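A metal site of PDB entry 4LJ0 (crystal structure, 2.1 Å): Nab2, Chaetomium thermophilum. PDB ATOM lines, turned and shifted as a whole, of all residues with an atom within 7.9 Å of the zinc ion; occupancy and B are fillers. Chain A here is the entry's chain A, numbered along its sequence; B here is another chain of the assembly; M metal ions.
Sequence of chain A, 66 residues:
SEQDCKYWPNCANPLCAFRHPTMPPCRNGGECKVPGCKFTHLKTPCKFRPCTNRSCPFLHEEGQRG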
ATOM      1  N   GLN A   3     -33.538  17.941  10.177  1.00  0.00           N
ATOM      2  CA  GLN A   3     -33.248  16.518  10.336  1.00  0.00           C
ATOM      3  C   GLN A   3     -33.427  16.122  11.788  1.00  0.00           C
ATOM      4  O   GLN A   3     -33.114  16.895  12.696  1.00  0.00           O
ATOM      5  CB  GLN A   3     -31.824  16.211   9.883  1.00  0.00           C
ATOM      6  CG  GLN A   3     -31.646  16.153   8.377  1.00  0.00           C
ATOM      7  CD  GLN A   3     -30.202  15.966   7.964  1.00  0.00           C
ATOM      8  OE1 GLN A   3     -29.499  16.938   7.687  1.00  0.00           O
ATOM      9  NE2 GLN A   3     -29.744  14.711   7.934  1.00  0.00           N
ATOM     10  N   ASP A   4     -33.941  14.917  12.015  1.00  0.00           N
ATOM     11  CA  ASP A   4     -34.130  14.402  13.366  1.00  0.00           C
ATOM     12  C   ASP A   4     -32.797  14.069  14.012  1.00  0.00           C
ATOM     13  O   ASP A   4     -31.928  13.459  13.387  1.00  0.00           O
ATOM     14  CB  ASP A   4     -34.986  13.140  13.349  1.00  0.00           C
ATOM     15  CG  ASP A   4     -36.423  13.415  12.955  1.00  0.00           C
ATOM     16  OD1 ASP A   4     -36.804  14.604  12.842  1.00  0.00           O
ATOM     17  OD2 ASP A   4     -37.183  12.437  12.778  1.00  0.00           O
ATOM     18  N   CYS A   5     -32.630  14.471  15.268  1.00  0.00           N
ATOM     19  CA  CYS A   5     -31.483  14.038  16.049  1.00  0.00           C
ATOM     20  C   CYS A   5     -31.546  12.513  16.168  1.00  0.00           C
ATOM     21  O   CYS A   5     -32.568  11.963  16.570  1.00  0.00           O
ATOM     22  CB  CYS A   5     -31.513  14.685  17.427  1.00  0.00           C
ATOM     23  SG  CYS A   5     -30.113  14.228  18.482  1.00  0.00           S
ATOM     24  N   LYS A   6     -30.463  11.838  15.803  1.00  0.00           N
ATOM     25  CA  LYS A   6     -30.437  10.379  15.836  1.00  0.00           C
ATOM     26  C   LYS A   6     -30.079   9.856  17.235  1.00  0.00           C
ATOM     27  O   LYS A   6     -30.080   8.651  17.461  1.00  0.00           O
ATOM     28  CB  LYS A   6     -29.450   9.825  14.808  1.00  0.00           C
ATOM     29  CG  LYS A   6     -27.985  10.069  15.110  1.00  0.00           C
ATOM     30  CD  LYS A   6     -27.079   9.427  14.062  1.00  0.00           C
ATOM     31  CE  LYS A   6     -25.603   9.655  14.381  1.00  0.00           C
ATOM     32  NZ  LYS A   6     -24.701   9.052  13.371  1.00  0.00           N
ATOM     33  N   TYR A   7     -29.785  10.776  18.149  1.00  0.00           N
ATOM     34  CA  TYR A   7     -29.354  10.400  19.495  1.00  0.00           C
ATOM     35  C   TYR A   7     -30.490  10.518  20.501  1.00  0.00           C
ATOM     36  O   TYR A   7     -30.509   9.822  21.510  1.00  0.00           O
ATOM     37  CB  TYR A   7     -28.176  11.277  19.926  1.00  0.00           C
ATOM     38  CG  TYR A   7     -26.953  11.060  19.074  1.00  0.00           C
ATOM     39  CD1 TYR A   7     -26.185   9.909  19.206  1.00  0.00           C
ATOM     40  CD2 TYR A   7     -26.558  12.009  18.132  1.00  0.00           C
ATOM     41  CE1 TYR A   7     -25.063   9.705  18.428  1.00  0.00           C
ATOM     42  CE2 TYR A   7     -25.436  11.805  17.354  1.00  0.00           C
ATOM     43  CZ  TYR A   7     -24.701  10.655  17.503  1.00  0.00           C
ATOM     44  OH  TYR A   7     -23.575  10.450  16.734  1.00  0.00           O
ATOM     45  N   TRP A   8     -31.442  11.402  20.214  1.00  0.00           N
ATOM     46  CA  TRP A   8     -32.623  11.549  21.042  1.00  0.00           C
ATOM     47  C   TRP A   8     -33.297  10.187  21.175  1.00  0.00           C
ATOM     48  O   TRP A   8     -33.366   9.444  20.190  1.00  0.00           O
ATOM     49  CB  TRP A   8     -33.588  12.565  20.410  1.00  0.00           C
ATOM     50  CG  TRP A   8     -34.725  12.933  21.304  1.00  0.00           C
ATOM     51  CD1 TRP A   8     -34.770  13.966  22.192  1.00  0.00           C
ATOM     52  CD2 TRP A   8     -35.977  12.241  21.412  1.00  0.00           C
ATOM     53  NE1 TRP A   8     -35.982  13.971  22.838  1.00  0.00           N
ATOM     54  CE2 TRP A   8     -36.741  12.926  22.378  1.00  0.00           C
ATOM     55  CE3 TRP A   8     -36.531  11.128  20.789  1.00  0.00           C
ATOM     56  CZ2 TRP A   8     -38.022  12.531  22.739  1.00  0.00           C
ATOM     57  CZ3 TRP A   8     -37.805  10.736  21.134  1.00  0.00           C
ATOM     58  CH2 TRP A   8     -38.546  11.432  22.101  1.00  0.00           C
ATOM     59  N   ASN A  10     -31.482  10.260  23.861  1.00  0.00           N
ATOM     60  CA  ASN A  10     -30.207  10.204  24.582  1.00  0.00           C
ATOM     61  C   ASN A  10     -29.181  11.146  23.972  1.00  0.00           C
ATOM     62  O   ASN A  10     -28.017  10.786  23.782  1.00  0.00           O
ATOM     63  CB  ASN A  10     -29.664   8.776  24.602  1.00  0.00           C
ATOM     64  CG  ASN A  10     -30.546   7.827  25.386  1.00  0.00           C
ATOM     65  OD1 ASN A  10     -30.991   6.797  24.868  1.00  0.00           O
ATOM     66  ND2 ASN A  10     -30.818   8.168  26.637  1.00  0.00           N
ATOM     67  N   CYS A  11     -29.621  12.356  23.666  1.00  0.00           N
ATOM     68  CA  CYS A  11     -28.755  13.377  23.106  1.00  0.00           C
ATOM     69  C   CYS A  11     -27.971  14.076  24.222  1.00  0.00           C
ATOM     70  O   CYS A  11     -28.574  14.570  25.177  1.00  0.00           O
ATOM     71  CB  CYS A  11     -29.573  14.403  22.321  1.00  0.00           C
ATOM     72  SG  CYS A  11     -28.567  15.639  21.499  1.00  0.00           S
ATOM     73  N   ALA A  12     -26.653  14.120  24.085  1.00  0.00           N
ATOM     74  CA  ALA A  12     -25.777  14.663  25.113  1.00  0.00           C
ATOM     75  C   ALA A  12     -25.299  16.075  24.801  1.00  0.00           C
ATOM     76  O   ALA A  12     -24.535  16.667  25.575  1.00  0.00           O
ATOM     77  CB  ALA A  12     -24.589  13.736  25.312  1.00  0.00           C
ATOM     78  N   ASN A  13     -25.723  16.615  23.661  1.00  0.00           N
ATOM     79  CA  ASN A  13     -25.322  17.954  23.261  1.00  0.00           C
ATOM     80  C   ASN A  13     -26.433  18.953  23.587  1.00  0.00           C
ATOM     81  O   ASN A  13     -27.447  19.006  22.891  1.00  0.00           O
ATOM     82  CB  ASN A  13     -25.014  17.986  21.761  1.00  0.00           C
ATOM     83  CG  ASN A  13     -24.460  19.319  21.295  1.00  0.00           C
ATOM     84  OD1 ASN A  13     -24.515  20.321  22.007  1.00  0.00           O
ATOM     85  ND2 ASN A  13     -23.921  19.342  20.081  1.00  0.00           N
ATOM     86  N   PRO A  14     -26.243  19.762  24.649  1.00  0.00           N
ATOM     87  CA  PRO A  14     -27.308  20.696  25.028  1.00  0.00           C
ATOM     88  C   PRO A  14     -27.601  21.757  23.957  1.00  0.00           C
ATOM     89  O   PRO A  14     -28.672  22.371  23.999  1.00  0.00           O
ATOM     90  CB  PRO A  14     -26.769  21.364  26.300  1.00  0.00           C
ATOM     91  CG  PRO A  14     -25.298  21.122  26.274  1.00  0.00           C
ATOM     92  CD  PRO A  14     -25.110  19.820  25.582  1.00  0.00           C
ATOM     93  N   LEU A  15     -26.674  21.953  23.027  1.00  0.00           N
ATOM     94  CA  LEU A  15     -26.857  22.930  21.952  1.00  0.00           C
ATOM     95  C   LEU A  15     -27.107  22.244  20.623  1.00  0.00           C
ATOM     96  O   LEU A  15     -26.873  22.824  19.567  1.00  0.00           O
ATOM     97  CB  LEU A  15     -25.635  23.834  21.835  1.00  0.00           C
ATOM     98  CG  LEU A  15     -25.200  24.581  23.107  1.00  0.00           C
ATOM     99  CD1 LEU A  15     -24.057  25.527  22.785  1.00  0.00           C
ATOM    100  CD2 LEU A  15     -26.361  25.343  23.739  1.00  0.00           C
ATOM    101  N   CYS A  16     -27.574  20.994  20.668  1.00  0.00           N
ATOM    102  CA  CYS A  16     -27.858  20.240  19.454  1.00  0.00           C
ATOM    103  C   CYS A  16     -28.839  21.008  18.594  1.00  0.00           C
ATOM    104  O   CYS A  16     -29.851  21.512  19.084  1.00  0.00           O
ATOM    105  CB  CYS A  16     -28.448  18.873  19.803  1.00  0.00           C
ATOM    106  SG  CYS A  16     -28.677  17.815  18.368  1.00  0.00           S
ATOM    107  N   ALA A  17     -28.531  21.108  17.299  1.00  0.00           N
ATOM    108  CA  ALA A  17     -29.341  21.880  16.364  1.00  0.00           C
ATOM    109  C   ALA A  17     -30.282  20.992  15.566  1.00  0.00           C
ATOM    110  O   ALA A  17     -31.107  21.476  14.794  1.00  0.00           O
ATOM    111  CB  ALA A  17     -28.443  22.654  15.430  1.00  0.00           C
ATOM    112  N   PHE A  18     -30.154  19.675  15.733  1.00  0.00           N
ATOM    113  CA  PHE A  18     -31.038  18.746  15.050  1.00  0.00           C
ATOM    114  C   PHE A  18     -32.375  18.687  15.791  1.00  0.00           C
ATOM    115  O   PHE A  18     -32.469  19.084  16.955  1.00  0.00           O
ATOM    116  CB  PHE A  18     -30.396  17.358  14.965  1.00  0.00           C
ATOM    117  CG  PHE A  18     -29.233  17.296  14.005  1.00  0.00           C
ATOM    118  CD1 PHE A  18     -27.993  17.810  14.366  1.00  0.00           C
ATOM    119  CD2 PHE A  18     -29.381  16.747  12.743  1.00  0.00           C
ATOM    120  CE1 PHE A  18     -26.927  17.760  13.489  1.00  0.00           C
ATOM    121  CE2 PHE A  18     -28.320  16.698  11.857  1.00  0.00           C
ATOM    122  CZ  PHE A  18     -27.088  17.208  12.233  1.00  0.00           C
ATOM    123  N   ARG A  19     -33.404  18.218  15.112  1.00  0.00           N
ATOM    124  CA  ARG A  19     -34.766  18.252  15.645  1.00  0.00           C
ATOM    125  C   ARG A  19     -34.952  17.278  16.804  1.00  0.00           C
ATOM    126  O   ARG A  19     -34.691  16.087  16.675  1.00  0.00           O
ATOM    127  CB  ARG A  19     -35.747  17.921  14.522  1.00  0.00           C
ATOM    128  CG  ARG A  19     -37.175  18.372  14.782  1.00  0.00           C
ATOM    129  CD  ARG A  19     -38.093  17.875  13.687  1.00  0.00           C
ATOM    130  NE  ARG A  19     -39.344  18.620  13.613  1.00  0.00           N
ATOM    131  CZ  ARG A  19     -40.303  18.388  12.719  1.00  0.00           C
ATOM    132  NH1 ARG A  19     -40.158  17.421  11.817  1.00  0.00           N
ATOM    133  NH2 ARG A  19     -41.412  19.114  12.729  1.00  0.00           N
ATOM    134  N   HIS A  20     -35.389  17.817  17.947  1.00  0.00           N
ATOM    135  CA  HIS A  20     -35.823  16.992  19.071  1.00  0.00           C
ATOM    136  C   HIS A  20     -37.324  17.149  19.242  1.00  0.00           C
ATOM    137  O   HIS A  20     -37.828  18.271  19.178  1.00  0.00           O
ATOM    138  CB  HIS A  20     -35.138  17.440  20.371  1.00  0.00           C
ATOM    139  CG  HIS A  20     -33.652  17.291  20.365  1.00  0.00           C
ATOM    140  ND1 HIS A  20     -32.896  17.357  21.511  1.00  0.00           N
ATOM    141  CD2 HIS A  20     -32.779  17.072  19.353  1.00  0.00           C
ATOM    142  CE1 HIS A  20     -31.626  17.190  21.209  1.00  0.00           C
ATOM    143  NE2 HIS A  20     -31.525  17.019  19.905  1.00  0.00           N
ATOM    144  P     A B   2     -18.296   9.596  19.903  1.00  0.00           P
ATOM    145  OP1   A B   2     -16.845   9.270  19.884  1.00  0.00           O
ATOM    146  OP2   A B   2     -19.206   8.911  18.941  1.00  0.00           O
ATOM    147  O5'   A B   2     -18.833   9.313  21.373  1.00  0.00           O
ATOM    148  C5'   A B   2     -19.933  10.044  21.905  1.00  0.00           C
ATOM    149  C4'   A B   2     -20.898   9.142  22.621  1.00  0.00           C
ATOM    150  O4'   A B   2     -22.028   9.944  23.072  1.00  0.00           O
ATOM    151  C3'   A B   2     -21.491   8.029  21.772  1.00  0.00           C
ATOM    152  O3'   A B   2     -21.779   6.893  22.595  1.00  0.00           O
ATOM    153  C2'   A B   2     -22.788   8.641  21.244  1.00  0.00           C
ATOM    154  O2'   A B   2     -23.780   7.715  20.896  1.00  0.00           O
ATOM    155  C1'   A B   2     -23.215   9.514  22.430  1.00  0.00           C
ATOM    156  N9    A B   2     -23.964  10.723  22.067  1.00  0.00           N
ATOM    157  C8    A B   2     -25.073  11.228  22.684  1.00  0.00           C
ATOM    158  N7    A B   2     -25.517  12.346  22.174  1.00  0.00           N
ATOM    159  C5    A B   2     -24.627  12.607  21.131  1.00  0.00           C
ATOM    160  C6    A B   2     -24.548  13.654  20.207  1.00  0.00           C
ATOM    161  N6    A B   2     -25.413  14.672  20.164  1.00  0.00           N
ATOM    162  N1    A B   2     -23.546  13.626  19.307  1.00  0.00           N
ATOM    163  C2    A B   2     -22.675  12.616  19.349  1.00  0.00           C
ATOM    164  N3    A B   2     -22.647  11.574  20.184  1.00  0.00           N
ATOM    165  C4    A B   2     -23.654  11.624  21.066  1.00  0.00           C
HETATM  166 ZN    ZN M   1     -29.785  16.145  19.637  1.00  0.00          ZN
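SG of Cys 11 lies close to N6 of A 2 of chain B (3.6 Å).
The side-chain sulfur of Cys 11 sits close to the backbone NH of Asn 13, 3.7 Å away.
The side-chain sulfur (SG) of Cys 5 lies close to the backbone NH (N) of Tyr 7 (3.5 Å).
SG of Cys 5 lies close to N of Trp 8, at 3.6 Å.
N of Phe 18 lies close to SG of Cys 16 (3.5 Å).
The backbone NH (N) of Cys 5 is in hydrogen-bond range of the backbone carbonyl oxygen (O) of Arg 19, 3.0 Å away.
OD1 of Asn 13 lies within hydrogen-bond range of N of Cys 16 (3.4 Å).
The nearest printed residue that does not touch the zinc ion is A 2 of chain B (4.6 Å).
The zinc ion is bound by NE2 of His 20 (2.0 Å), SG of Cys 5 (2.3 Å), SG of Cys 11 (2.3 Å) and SG of Cys 16 (2.4 Å).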
